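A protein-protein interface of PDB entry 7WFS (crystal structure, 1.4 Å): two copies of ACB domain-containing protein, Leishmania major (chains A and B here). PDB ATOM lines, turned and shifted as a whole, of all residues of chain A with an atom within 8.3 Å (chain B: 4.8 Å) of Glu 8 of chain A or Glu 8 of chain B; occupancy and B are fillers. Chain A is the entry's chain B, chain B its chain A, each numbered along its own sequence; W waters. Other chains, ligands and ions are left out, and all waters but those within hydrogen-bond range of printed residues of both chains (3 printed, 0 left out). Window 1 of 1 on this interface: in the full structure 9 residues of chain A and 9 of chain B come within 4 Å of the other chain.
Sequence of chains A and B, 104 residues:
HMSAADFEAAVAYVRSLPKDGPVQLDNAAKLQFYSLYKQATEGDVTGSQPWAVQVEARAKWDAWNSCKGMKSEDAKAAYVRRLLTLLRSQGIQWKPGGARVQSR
The side-chain amino group (NZ) of Lys 76 of chain B lies within hydrogen-bond range of the side-chain hydroxyl (OH) of Tyr 37 of chain A, 3.3 Å away.
OE2 of Glu 8 of chain B lies within hydrogen-bond range of OH of Tyr 37 of chain A.
The side-chain carboxylate of Asp 6 of chain B is in salt-bridge range of the guanidinium group of Arg 15 of chain A (3.3 Å).
O of Ala 5 of chain B is in hydrogen-bond range of NE of Arg 15 of chain A (3.3 Å).
The side-chain carboxylate (OE2) of Glu 8 of chain A lies within hydrogen-bond range of the side-chain hydroxyl (OH) of Tyr 37 of chain B, at 2.6 Å.
The side-chain hydroxyl of Tyr 37 of chain B is in hydrogen-bond range of the side-chain amino group of Lys 76 of chain A (3.3 Å).
The backbone carbonyl oxygen (O) of Tyr 37 of chain B sits at hydrogen-bond distance from the side-chain hydroxyl (OG1) of Thr 41 of chain B.
OE1 of Glu 73 of chain A is in salt-bridge range of NZ of Lys 76 of chain A, 2.9 Å away.
The side-chain hydroxyl of Thr 41 of chain A lies within hydrogen-bond range of the backbone carbonyl oxygen of Tyr 37 of chain A (2.7 Å).
Among the printed residues, merely in contact across the chains: Glu 8 of chain A with Glu 8 of chain B, Glu 8 of chain A with Val 11 of chain B, Ala 9 of chain A with Ala 12 of chain B, Val 11 of chain A with Glu 8 of chain B and Ala 12 of chain A with Ala 9 of chain B.
Glu 8 of chain A touches three residues of chain B.
Glu 8 of chain B touches just these residues of chain A: Glu 8, Val 11 and Tyr 37.
Of chain A, only Ala 12 comes within 4 Å of Ala 9 of chain B.
Printed residues of chain A within 4 Å of Lys 76 of chain B: Tyr 37.
Of the printed residues of chain B, Ala 9 of chain A touches Ala 12 (3.5 Å).
Of the printed residues of chain A, Val 11 of chain B touches Glu 8.
Printed residues of chain B within 4 Å of Ala 12 of chain A: Ala 9.
Of the printed residues of chain A, Tyr 37 of chain B touches Glu 8 (2.6 Å) and Lys 76 (3.3 Å).
Ala 4 of chain B touches none of the printed residues of chain A.
Ser 3 of chain A touches none of the printed residues of chain B.
The nearest residue of chain A that does not touch Glu 8 of chain B is Ala 12 of chain A (4.2 Å).
Of the 12 printed residues of chain B, 8 touch a printed residue of chain A.
Hydrophobic or aromatic side chains of chain B that line the printed part of chain A: Ala 5, Ala 9, Val 11, Ala 12 and Tyr 37.
Among the printed residues, 11 pairs touch across the chains.
Glu 8 of chain A touches Val 11 of chain B, and with the chains exchanged Val 11 of chain A touches Glu 8 of chain B.
Glu 8 of chain A touches Tyr 37 of chain B, and with the chains exchanged Tyr 37 of chain A touches Glu 8 of chain B.
Ala 9 of chain A touches Ala 12 of chain B, and with the chains exchanged Ala 12 of chain A touches Ala 9 of chain B.
Tyr 37 of chain A touches Lys 76 of chain B, and with the chains exchanged Lys 76 of chain A touches Tyr 37 of chain B.
12 positions are printed for both chains.
Water W3 lies within hydrogen-bond range of the side-chain carboxylate (OE1) of Glu 8 of chain B (2.7 Å), the backbone carbonyl oxygen (O) of Ala 4 of chain B (2.8 Å), the side-chain amino group (NZ) of Lys 76 of chain B (2.9 Å) and the side-chain hydroxyl (OH) of Tyr 37 of chain A (3.4 Å).
Water W2 lies within hydrogen-bond range of O of Ala 4 of chain A (2.8 Å), OE1 of Glu 8 of chain A (2.8 Å), NZ of Lys 76 of chain A (2.9 Å) and OH of Tyr 37 of chain B (3.4 Å).
Water W1 bridges the guanidinium group (NE) of Arg 15 of chain A and the side-chain carboxylate (OD1) of Asp 6 of chain B.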
ATOM      1  N   SER A   3      -4.585 -16.036 -14.993  1.00  0.00           N
ATOM      2  CA  SER A   3      -4.683 -16.559 -13.651  1.00  0.00           C
ATOM      3  C   SER A   3      -4.645 -18.066 -13.766  1.00  0.00           C
ATOM      4  O   SER A   3      -4.506 -18.623 -14.863  1.00  0.00           O
ATOM      5  CB  SER A   3      -6.012 -16.133 -13.016  1.00  0.00           C
ATOM      6  OG  SER A   3      -7.096 -16.575 -13.819  1.00  0.00           O
ATOM      7  N   ALA A   4      -4.809 -18.727 -12.625  1.00  0.00           N
ATOM      8  CA  ALA A   4      -5.002 -20.169 -12.642  1.00  0.00           C
ATOM      9  C   ALA A   4      -6.202 -20.580 -13.489  1.00  0.00           C
ATOM     10  O   ALA A   4      -6.286 -21.758 -13.860  1.00  0.00           O
ATOM     11  CB  ALA A   4      -5.168 -20.691 -11.213  1.00  0.00           C
ATOM     12  N   ALA A   5      -7.128 -19.651 -13.783  1.00  0.00           N
ATOM     13  CA  ALA A   5      -8.301 -19.999 -14.581  1.00  0.00           C
ATOM     14  C   ALA A   5      -7.925 -20.339 -16.006  1.00  0.00           C
ATOM     15  O   ALA A   5      -8.715 -20.962 -16.726  1.00  0.00           O
ATOM     16  CB  ALA A   5      -9.304 -18.854 -14.588  1.00  0.00           C
ATOM     17  N   ASP A   6      -6.742 -19.916 -16.429  1.00  0.00           N
ATOM     18  CA  ASP A   6      -6.248 -20.202 -17.766  1.00  0.00           C
ATOM     19  C   ASP A   6      -5.410 -21.460 -17.809  1.00  0.00           C
ATOM     20  O   ASP A   6      -4.772 -21.739 -18.819  1.00  0.00           O
ATOM     21  CB  ASP A   6      -5.433 -19.020 -18.269  1.00  0.00           C
ATOM     22  CG  ASP A   6      -6.251 -17.759 -18.346  1.00  0.00           C
ATOM     23  OD1 ASP A   6      -7.191 -17.737 -19.156  1.00  0.00           O
ATOM     24  OD2 ASP A   6      -5.983 -16.823 -17.557  1.00  0.00           O
ATOM     25  N   PHE A   7      -5.379 -22.219 -16.720  1.00  0.00           N
ATOM     26  CA  PHE A   7      -4.600 -23.453 -16.708  1.00  0.00           C
ATOM     27  C   PHE A   7      -5.012 -24.399 -17.826  1.00  0.00           C
ATOM     28  O   PHE A   7      -4.161 -24.967 -18.518  1.00  0.00           O
ATOM     29  CB  PHE A   7      -4.856 -24.141 -15.365  1.00  0.00           C
ATOM     30  CG  PHE A   7      -4.323 -25.534 -15.261  1.00  0.00           C
ATOM     31  CD1 PHE A   7      -2.960 -25.777 -15.162  1.00  0.00           C
ATOM     32  CD2 PHE A   7      -5.189 -26.629 -15.193  1.00  0.00           C
ATOM     33  CE1 PHE A   7      -2.489 -27.083 -14.985  1.00  0.00           C
ATOM     34  CE2 PHE A   7      -4.727 -27.937 -15.023  1.00  0.00           C
ATOM     35  CZ  PHE A   7      -3.355 -28.169 -14.934  1.00  0.00           C
ATOM     36  N   GLU A   8      -6.318 -24.563 -18.046  1.00  0.00           N
ATOM     37  CA  GLU A   8      -6.754 -25.504 -19.076  1.00  0.00           C
ATOM     38  C   GLU A   8      -6.298 -25.058 -20.467  1.00  0.00           C
ATOM     39  O   GLU A   8      -5.868 -25.880 -21.273  1.00  0.00           O
ATOM     40  CB  GLU A   8      -8.275 -25.674 -18.997  1.00  0.00           C
ATOM     41  CG  GLU A   8      -8.731 -26.517 -17.777  1.00  0.00           C
ATOM     42  CD  GLU A   8      -8.907 -25.730 -16.500  1.00  0.00           C
ATOM     43  OE1 GLU A   8      -8.694 -24.497 -16.478  1.00  0.00           O
ATOM     44  OE2 GLU A   8      -9.299 -26.378 -15.478  1.00  0.00           O
ATOM     45  N   ALA A   9      -6.406 -23.763 -20.757  1.00  0.00           N
ATOM     46  CA  ALA A   9      -5.934 -23.241 -22.036  1.00  0.00           C
ATOM     47  C   ALA A   9      -4.448 -23.508 -22.182  1.00  0.00           C
ATOM     48  O   ALA A   9      -3.966 -23.819 -23.280  1.00  0.00           O
ATOM     49  CB  ALA A   9      -6.204 -21.739 -22.095  1.00  0.00           C
ATOM     50  N   ALA A  10      -3.696 -23.341 -21.090  1.00  0.00           N
ATOM     51  CA  ALA A  10      -2.247 -23.558 -21.175  1.00  0.00           C
ATOM     52  C   ALA A  10      -1.934 -25.026 -21.430  1.00  0.00           C
ATOM     53  O   ALA A  10      -1.030 -25.352 -22.218  1.00  0.00           O
ATOM     54  CB  ALA A  10      -1.578 -23.096 -19.875  1.00  0.00           C
ATOM     55  N   VAL A  11      -2.663 -25.927 -20.753  1.00  0.00           N
ATOM     56  CA  VAL A  11      -2.485 -27.366 -20.979  1.00  0.00           C
ATOM     57  C   VAL A  11      -2.812 -27.703 -22.412  1.00  0.00           C
ATOM     58  O   VAL A  11      -2.057 -28.408 -23.092  1.00  0.00           O
ATOM     59  CB  VAL A  11      -3.335 -28.192 -20.000  1.00  0.00           C
ATOM     60  CG1 VAL A  11      -3.358 -29.663 -20.456  1.00  0.00           C
ATOM     61  CG2 VAL A  11      -2.790 -28.013 -18.607  1.00  0.00           C
ATOM     62  N   ALA A  12      -3.923 -27.161 -22.910  1.00  0.00           N
ATOM     63  CA  ALA A  12      -4.316 -27.468 -24.274  1.00  0.00           C
ATOM     64  C   ALA A  12      -3.266 -26.956 -25.246  1.00  0.00           C
ATOM     65  O   ALA A  12      -2.973 -27.610 -26.253  1.00  0.00           O
ATOM     66  CB  ALA A  12      -5.697 -26.894 -24.567  1.00  0.00           C
ATOM     67  N   TYR A  13      -2.684 -25.791 -24.935  1.00  0.00           N
ATOM     68  CA  TYR A  13      -1.647 -25.227 -25.799  1.00  0.00           C
ATOM     69  C   TYR A  13      -0.436 -26.154 -25.859  1.00  0.00           C
ATOM     70  O   TYR A  13       0.032 -26.518 -26.945  1.00  0.00           O
ATOM     71  CB  TYR A  13      -1.260 -23.831 -25.298  1.00  0.00           C
ATOM     72  CG  TYR A  13      -0.164 -23.183 -26.124  1.00  0.00           C
ATOM     73  CD1 TYR A  13      -0.478 -22.369 -27.214  1.00  0.00           C
ATOM     74  CD2 TYR A  13       1.172 -23.404 -25.879  1.00  0.00           C
ATOM     75  CE1 TYR A  13       0.506 -21.804 -27.973  1.00  0.00           C
ATOM     76  CE2 TYR A  13       2.156 -22.822 -26.672  1.00  0.00           C
ATOM     77  CZ  TYR A  13       1.814 -22.029 -27.693  1.00  0.00           C
ATOM     78  OH  TYR A  13       2.787 -21.430 -28.491  1.00  0.00           O
ATOM     79  N   VAL A  14       0.070 -26.573 -24.700  1.00  0.00           N
ATOM     80  CA  VAL A  14       1.208 -27.497 -24.659  1.00  0.00           C
ATOM     81  C   VAL A  14       0.899 -28.780 -25.409  1.00  0.00           C
ATOM     82  O   VAL A  14       1.725 -29.269 -26.187  1.00  0.00           O
ATOM     83  CB  VAL A  14       1.603 -27.773 -23.202  1.00  0.00           C
ATOM     84  CG1 VAL A  14       2.696 -28.851 -23.137  1.00  0.00           C
ATOM     85  CG2 VAL A  14       2.075 -26.471 -22.570  1.00  0.00           C
ATOM     86  N   ARG A  15      -0.310 -29.328 -25.216  1.00  0.00           N
ATOM     87  CA  ARG A  15      -0.680 -30.564 -25.904  1.00  0.00           C
ATOM     88  C   ARG A  15      -0.685 -30.385 -27.408  1.00  0.00           C
ATOM     89  O   ARG A  15      -0.487 -31.353 -28.156  1.00  0.00           O
ATOM     90  CB  ARG A  15      -2.065 -31.030 -25.445  1.00  0.00           C
ATOM     91  CG  ARG A  15      -2.031 -31.787 -24.131  1.00  0.00           C
ATOM     92  CD  ARG A  15      -3.407 -32.307 -23.736  1.00  0.00           C
ATOM     93  NE  ARG A  15      -4.090 -32.880 -24.894  1.00  0.00           N
ATOM     94  CZ  ARG A  15      -4.014 -34.157 -25.265  1.00  0.00           C
ATOM     95  NH1 ARG A  15      -3.288 -35.019 -24.566  1.00  0.00           N
ATOM     96  NH2 ARG A  15      -4.671 -34.578 -26.333  1.00  0.00           N
ATOM     97  N   TYR A  37       1.201 -30.289 -13.617  1.00  0.00           N
ATOM     98  CA  TYR A  37      -0.094 -30.776 -14.115  1.00  0.00           C
ATOM     99  C   TYR A  37      -0.699 -31.799 -13.160  1.00  0.00           C
ATOM    100  O   TYR A  37      -1.897 -31.746 -12.857  1.00  0.00           O
ATOM    101  CB  TYR A  37       0.045 -31.381 -15.521  1.00  0.00           C
ATOM    102  CG  TYR A  37      -1.273 -31.949 -16.012  1.00  0.00           C
ATOM    103  CD1 TYR A  37      -2.269 -31.105 -16.501  1.00  0.00           C
ATOM    104  CD2 TYR A  37      -1.557 -33.324 -15.917  1.00  0.00           C
ATOM    105  CE1 TYR A  37      -3.521 -31.625 -16.899  1.00  0.00           C
ATOM    106  CE2 TYR A  37      -2.786 -33.834 -16.327  1.00  0.00           C
ATOM    107  CZ  TYR A  37      -3.740 -32.982 -16.836  1.00  0.00           C
ATOM    108  OH  TYR A  37      -4.972 -33.465 -17.252  1.00  0.00           O
ATOM    109  N   ALA A  40      -1.751 -30.184  -9.884  1.00  0.00           N
ATOM    110  CA  ALA A  40      -2.932 -29.353 -10.085  1.00  0.00           C
ATOM    111  C   ALA A  40      -4.212 -30.179 -10.197  1.00  0.00           C
ATOM    112  O   ALA A  40      -5.291 -29.719  -9.810  1.00  0.00           O
ATOM    113  CB  ALA A  40      -2.748 -28.596 -11.396  1.00  0.00           C
ATOM    114  N   THR A  41      -4.135 -31.349 -10.821  1.00  0.00           N
ATOM    115  CA  THR A  41      -5.332 -32.097 -11.185  1.00  0.00           C
ATOM    116  C   THR A  41      -5.612 -33.300 -10.303  1.00  0.00           C
ATOM    117  O   THR A  41      -6.776 -33.745 -10.236  1.00  0.00           O
ATOM    118  CB  THR A  41      -5.217 -32.601 -12.635  1.00  0.00           C
ATOM    119  OG1 THR A  41      -4.049 -33.413 -12.759  1.00  0.00           O
ATOM    120  CG2 THR A  41      -5.129 -31.445 -13.615  1.00  0.00           C
ATOM    121  N   SER A  72      -3.786 -26.951  -5.192  1.00  0.00           N
ATOM    122  CA  SER A  72      -4.092 -27.185  -6.608  1.00  0.00           C
ATOM    123  C   SER A  72      -4.048 -25.888  -7.401  1.00  0.00           C
ATOM    124  O   SER A  72      -3.455 -25.828  -8.491  1.00  0.00           O
ATOM    125  CB  SER A  72      -5.475 -27.823  -6.747  1.00  0.00           C
ATOM    126  OG  SER A  72      -5.887 -27.802  -8.105  1.00  0.00           O
ATOM    127  N   GLU A  73      -4.666 -24.823  -6.877  1.00  0.00           N
ATOM    128  CA  GLU A  73      -4.686 -23.562  -7.642  1.00  0.00           C
ATOM    129  C   GLU A  73      -3.298 -22.954  -7.784  1.00  0.00           C
ATOM    130  O   GLU A  73      -3.024 -22.247  -8.764  1.00  0.00           O
ATOM    131  CB  GLU A  73      -5.662 -22.579  -6.985  1.00  0.00           C
ATOM    132  CG  GLU A  73      -7.135 -23.002  -7.102  1.00  0.00           C
ATOM    133  CD  GLU A  73      -7.619 -23.093  -8.544  1.00  0.00           C
ATOM    134  OE1 GLU A  73      -8.136 -24.168  -8.951  1.00  0.00           O
ATOM    135  OE2 GLU A  73      -7.464 -22.092  -9.277  1.00  0.00           O
ATOM    136  N   LYS A  76      -1.712 -24.858 -10.594  1.00  0.00           N
ATOM    137  CA  LYS A  76      -2.222 -24.335 -11.867  1.00  0.00           C
ATOM    138  C   LYS A  76      -1.534 -23.033 -12.201  1.00  0.00           C
ATOM    139  O   LYS A  76      -1.117 -22.830 -13.351  1.00  0.00           O
ATOM    140  CB  LYS A  76      -3.737 -24.099 -11.779  1.00  0.00           C
ATOM    141  CG  LYS A  76      -4.597 -25.336 -11.653  1.00  0.00           C
ATOM    142  CD  LYS A  76      -6.052 -24.852 -11.605  1.00  0.00           C
ATOM    143  CE  LYS A  76      -7.059 -25.954 -11.687  1.00  0.00           C
ATOM    144  NZ  LYS A  76      -8.453 -25.382 -11.573  1.00  0.00           N
ATOM    145  N   TYR A  79       2.002 -23.625 -13.412  1.00  0.00           N
ATOM    146  CA  TYR A  79       2.020 -24.183 -14.756  1.00  0.00           C
ATOM    147  C   TYR A  79       1.865 -23.072 -15.782  1.00  0.00           C
ATOM    148  O   TYR A  79       2.624 -23.002 -16.752  1.00  0.00           O
ATOM    149  CB  TYR A  79       0.904 -25.215 -14.911  1.00  0.00           C
ATOM    150  CG  TYR A  79       0.898 -25.998 -16.215  1.00  0.00           C
ATOM    151  CD1 TYR A  79       1.247 -27.337 -16.245  1.00  0.00           C
ATOM    152  CD2 TYR A  79       0.540 -25.387 -17.430  1.00  0.00           C
ATOM    153  CE1 TYR A  79       1.257 -28.072 -17.383  1.00  0.00           C
ATOM    154  CE2 TYR A  79       0.543 -26.109 -18.621  1.00  0.00           C
ATOM    155  CZ  TYR A  79       0.887 -27.433 -18.611  1.00  0.00           C
ATOM    156  OH  TYR A  79       0.876 -28.148 -19.777  1.00  0.00           O
ATOM    157  N   VAL A  80       0.889 -22.196 -15.593  1.00  0.00           N
ATOM    158  CA  VAL A  80       0.686 -21.148 -16.596  1.00  0.00           C
ATOM    159  C   VAL A  80       1.901 -20.229 -16.651  1.00  0.00           C
ATOM    160  O   VAL A  80       2.388 -19.871 -17.734  1.00  0.00           O
ATOM    161  CB  VAL A  80      -0.616 -20.381 -16.308  1.00  0.00           C
ATOM    162  CG1 VAL A  80      -0.854 -19.313 -17.350  1.00  0.00           C
ATOM    163  CG2 VAL A  80      -1.790 -21.313 -16.307  1.00  0.00           C
ATOM    164  N   LEU A  83       4.690 -21.803 -18.536  1.00  0.00           N
ATOM    165  CA  LEU A  83       4.499 -21.736 -19.986  1.00  0.00           C
ATOM    166  C   LEU A  83       4.832 -20.336 -20.492  1.00  0.00           C
ATOM    167  O   LEU A  83       5.519 -20.168 -21.516  1.00  0.00           O
ATOM    168  CB  LEU A  83       3.058 -22.131 -20.338  1.00  0.00           C
ATOM    169  CG  LEU A  83       2.738 -21.975 -21.832  1.00  0.00           C
ATOM    170  CD1 LEU A  83       3.567 -22.935 -22.662  1.00  0.00           C
ATOM    171  CD2 LEU A  83       1.231 -22.231 -21.995  1.00  0.00           C
ATOM    172  N   TRP A  94       2.256 -15.588 -25.751  1.00  0.00           N
ATOM    173  CA  TRP A  94       1.006 -16.328 -25.809  1.00  0.00           C
ATOM    174  C   TRP A  94      -0.048 -15.661 -24.940  1.00  0.00           C
ATOM    175  O   TRP A  94       0.265 -15.009 -23.940  1.00  0.00           O
ATOM    176  CB  TRP A  94       1.190 -17.771 -25.338  1.00  0.00           C
ATOM    177  CG  TRP A  94      -0.073 -18.616 -25.315  1.00  0.00           C
ATOM    178  CD1 TRP A  94      -0.756 -19.096 -26.392  1.00  0.00           C
ATOM    179  CD2 TRP A  94      -0.790 -19.066 -24.154  1.00  0.00           C
ATOM    180  NE1 TRP A  94      -1.854 -19.819 -25.976  1.00  0.00           N
ATOM    181  CE2 TRP A  94      -1.887 -19.824 -24.606  1.00  0.00           C
ATOM    182  CE3 TRP A  94      -0.605 -18.906 -22.777  1.00  0.00           C
ATOM    183  CZ2 TRP A  94      -2.799 -20.416 -23.734  1.00  0.00           C
ATOM    184  CZ3 TRP A  94      -1.511 -19.511 -21.910  1.00  0.00           C
ATOM    185  CH2 TRP A  94      -2.592 -20.243 -22.394  1.00  0.00           C
ATOM    186  N   PRO A  96      -4.577 -16.840 -24.273  1.00  0.00           N
ATOM    187  CA  PRO A  96      -5.634 -17.751 -24.725  1.00  0.00           C
ATOM    188  C   PRO A  96      -6.325 -17.243 -25.985  1.00  0.00           C
ATOM    189  O   PRO A  96      -6.466 -16.038 -26.203  1.00  0.00           O
ATOM    190  CB  PRO A  96      -6.606 -17.780 -23.539  1.00  0.00           C
ATOM    191  CG  PRO A  96      -5.767 -17.465 -22.361  1.00  0.00           C
ATOM    192  CD  PRO A  96      -4.709 -16.502 -22.846  1.00  0.00           C
ATOM    193  N   ALA B   4     -10.935 -38.042 -22.930  1.00  0.00           N
ATOM    194  CA  ALA B   4     -10.770 -37.206 -21.746  1.00  0.00           C
ATOM    195  C   ALA B   4      -9.502 -36.360 -21.805  1.00  0.00           C
ATOM    196  O   ALA B   4      -9.406 -35.372 -21.071  1.00  0.00           O
ATOM    197  CB  ALA B   4     -10.721 -38.086 -20.498  1.00  0.00           C
ATOM    198  N   ALA B   5      -8.521 -36.747 -22.619  1.00  0.00           N
ATOM    199  CA  ALA B   5      -7.293 -35.967 -22.725  1.00  0.00           C
ATOM    200  C   ALA B   5      -7.558 -34.584 -23.295  1.00  0.00           C
ATOM    201  O   ALA B   5      -6.772 -33.654 -23.063  1.00  0.00           O
ATOM    202  CB  ALA B   5      -6.278 -36.698 -23.602  1.00  0.00           C
ATOM    203  N   ASP B   6      -8.645 -34.423 -24.033  1.00  0.00           N
ATOM    204  CA  ASP B   6      -8.985 -33.120 -24.586  1.00  0.00           C
ATOM    205  C   ASP B   6      -9.852 -32.304 -23.644  1.00  0.00           C
ATOM    206  O   ASP B   6     -10.340 -31.249 -24.018  1.00  0.00           O
ATOM    207  CB  ASP B   6      -9.694 -33.324 -25.911  1.00  0.00           C
ATOM    208  CG  ASP B   6      -8.828 -34.081 -26.896  1.00  0.00           C
ATOM    209  OD1 ASP B   6      -7.734 -33.571 -27.230  1.00  0.00           O
ATOM    210  OD2 ASP B   6      -9.199 -35.210 -27.282  1.00  0.00           O
ATOM    211  N   PHE B   7     -10.029 -32.760 -22.406  1.00  0.00           N
ATOM    212  CA  PHE B   7     -10.856 -32.026 -21.465  1.00  0.00           C
ATOM    213  C   PHE B   7     -10.387 -30.584 -21.323  1.00  0.00           C
ATOM    214  O   PHE B   7     -11.189 -29.652 -21.340  1.00  0.00           O
ATOM    215  CB  PHE B   7     -10.807 -32.777 -20.134  1.00  0.00           C
ATOM    216  CG  PHE B   7     -11.402 -32.033 -18.982  1.00  0.00           C
ATOM    217  CD1 PHE B   7     -12.781 -31.889 -18.888  1.00  0.00           C
ATOM    218  CD2 PHE B   7     -10.590 -31.487 -17.987  1.00  0.00           C
ATOM    219  CE1 PHE B   7     -13.362 -31.218 -17.796  1.00  0.00           C
ATOM    220  CE2 PHE B   7     -11.134 -30.827 -16.871  1.00  0.00           C
ATOM    221  CZ  PHE B   7     -12.538 -30.664 -16.790  1.00  0.00           C
ATOM    222  N   GLU B   8      -9.089 -30.388 -21.153  1.00  0.00           N
ATOM    223  CA  GLU B   8      -8.592 -29.032 -20.962  1.00  0.00           C
ATOM    224  C   GLU B   8      -8.924 -28.160 -22.164  1.00  0.00           C
ATOM    225  O   GLU B   8      -9.291 -26.997 -22.006  1.00  0.00           O
ATOM    226  CB  GLU B   8      -7.080 -29.073 -20.695  1.00  0.00           C
ATOM    227  CG  GLU B   8      -6.794 -29.601 -19.262  1.00  0.00           C
ATOM    228  CD  GLU B   8      -6.735 -31.122 -19.135  1.00  0.00           C
ATOM    229  OE1 GLU B   8      -6.852 -31.842 -20.125  1.00  0.00           O
ATOM    230  OE2 GLU B   8      -6.559 -31.604 -17.979  1.00  0.00           O
ATOM    231  N   ALA B   9      -8.786 -28.711 -23.365  1.00  0.00           N
ATOM    232  CA  ALA B   9      -9.100 -27.931 -24.562  1.00  0.00           C
ATOM    233  C   ALA B   9     -10.580 -27.574 -24.603  1.00  0.00           C
ATOM    234  O   ALA B   9     -10.964 -26.473 -25.049  1.00  0.00           O
ATOM    235  CB  ALA B   9      -8.715 -28.730 -25.809  1.00  0.00           C
ATOM    236  N   ALA B  10     -11.435 -28.522 -24.219  1.00  0.00           N
ATOM    237  CA  ALA B  10     -12.863 -28.237 -24.215  1.00  0.00           C
ATOM    238  C   ALA B  10     -13.186 -27.152 -23.197  1.00  0.00           C
ATOM    239  O   ALA B  10     -13.978 -26.241 -23.471  1.00  0.00           O
ATOM    240  CB  ALA B  10     -13.614 -29.518 -23.881  1.00  0.00           C
ATOM    241  N   VAL B  11     -12.626 -27.269 -21.985  1.00  0.00           N
ATOM    242  CA  VAL B  11     -12.828 -26.204 -20.994  1.00  0.00           C
ATOM    243  C   VAL B  11     -12.374 -24.857 -21.537  1.00  0.00           C
ATOM    244  O   VAL B  11     -13.080 -23.849 -21.423  1.00  0.00           O
ATOM    245  CB  VAL B  11     -12.099 -26.544 -19.683  1.00  0.00           C
ATOM    246  CG1 VAL B  11     -12.081 -25.337 -18.742  1.00  0.00           C
ATOM    247  CG2 VAL B  11     -12.746 -27.762 -19.065  1.00  0.00           C
ATOM    248  N   ALA B  12     -11.151 -24.798 -22.089  1.00  0.00           N
ATOM    249  CA  ALA B  12     -10.655 -23.513 -22.572  1.00  0.00           C
ATOM    250  C   ALA B  12     -11.580 -22.964 -23.653  1.00  0.00           C
ATOM    251  O   ALA B  12     -11.809 -21.756 -23.724  1.00  0.00           O
ATOM    252  CB  ALA B  12      -9.227 -23.669 -23.110  1.00  0.00           C
ATOM    253  N   TYR B  37     -17.270 -30.282 -14.597  1.00  0.00           N
ATOM    254  CA  TYR B  37     -15.954 -29.677 -14.441  1.00  0.00           C
ATOM    255  C   TYR B  37     -15.488 -29.837 -13.008  1.00  0.00           C
ATOM    256  O   TYR B  37     -14.338 -30.191 -12.752  1.00  0.00           O
ATOM    257  CB  TYR B  37     -16.019 -28.191 -14.786  1.00  0.00           C
ATOM    258  CG  TYR B  37     -14.698 -27.515 -14.513  1.00  0.00           C
ATOM    259  CD1 TYR B  37     -13.626 -27.658 -15.399  1.00  0.00           C
ATOM    260  CD2 TYR B  37     -14.501 -26.760 -13.369  1.00  0.00           C
ATOM    261  CE1 TYR B  37     -12.385 -27.046 -15.118  1.00  0.00           C
ATOM    262  CE2 TYR B  37     -13.273 -26.159 -13.082  1.00  0.00           C
ATOM    263  CZ  TYR B  37     -12.227 -26.295 -13.966  1.00  0.00           C
ATOM    264  OH  TYR B  37     -11.018 -25.685 -13.641  1.00  0.00           O
ATOM    265  N   THR B  41     -12.311 -32.131 -11.774  1.00  0.00           N
ATOM    266  CA  THR B  41     -11.120 -31.470 -11.241  1.00  0.00           C
ATOM    267  C   THR B  41     -11.021 -31.494  -9.731  1.00  0.00           C
ATOM    268  O   THR B  41      -9.936 -31.209  -9.199  1.00  0.00           O
ATOM    269  CB  THR B  41     -11.089 -29.993 -11.653  1.00  0.00           C
ATOM    270  OG1 THR B  41     -12.298 -29.347 -11.231  1.00  0.00           O
ATOM    271  CG2 THR B  41     -10.958 -29.868 -13.166  1.00  0.00           C
ATOM    272  N   LYS B  76     -14.421 -36.068 -17.110  1.00  0.00           N
ATOM    273  CA  LYS B  76     -13.771 -35.324 -18.196  1.00  0.00           C
ATOM    274  C   LYS B  76     -14.368 -35.731 -19.526  1.00  0.00           C
ATOM    275  O   LYS B  76     -14.680 -34.871 -20.363  1.00  0.00           O
ATOM    276  CB  LYS B  76     -12.265 -35.612 -18.221  1.00  0.00           C
ATOM    277  CG  LYS B  76     -11.459 -35.047 -17.075  1.00  0.00           C
ATOM    278  CD  LYS B  76     -10.006 -35.451 -17.308  1.00  0.00           C
ATOM    279  CE  LYS B  76      -9.028 -34.816 -16.355  1.00  0.00           C
ATOM    280  NZ  LYS B  76      -7.625 -35.305 -16.686  1.00  0.00           N
HETATM  281  O   HOH W   1      -6.053 -31.190 -26.126  1.00  0.00           O
HETATM  282  O   HOH W   2      -8.346 -23.639 -13.837  1.00  0.00           O
HETATM  283  O   HOH W   3      -7.365 -34.435 -19.409  1.00  0.00           O
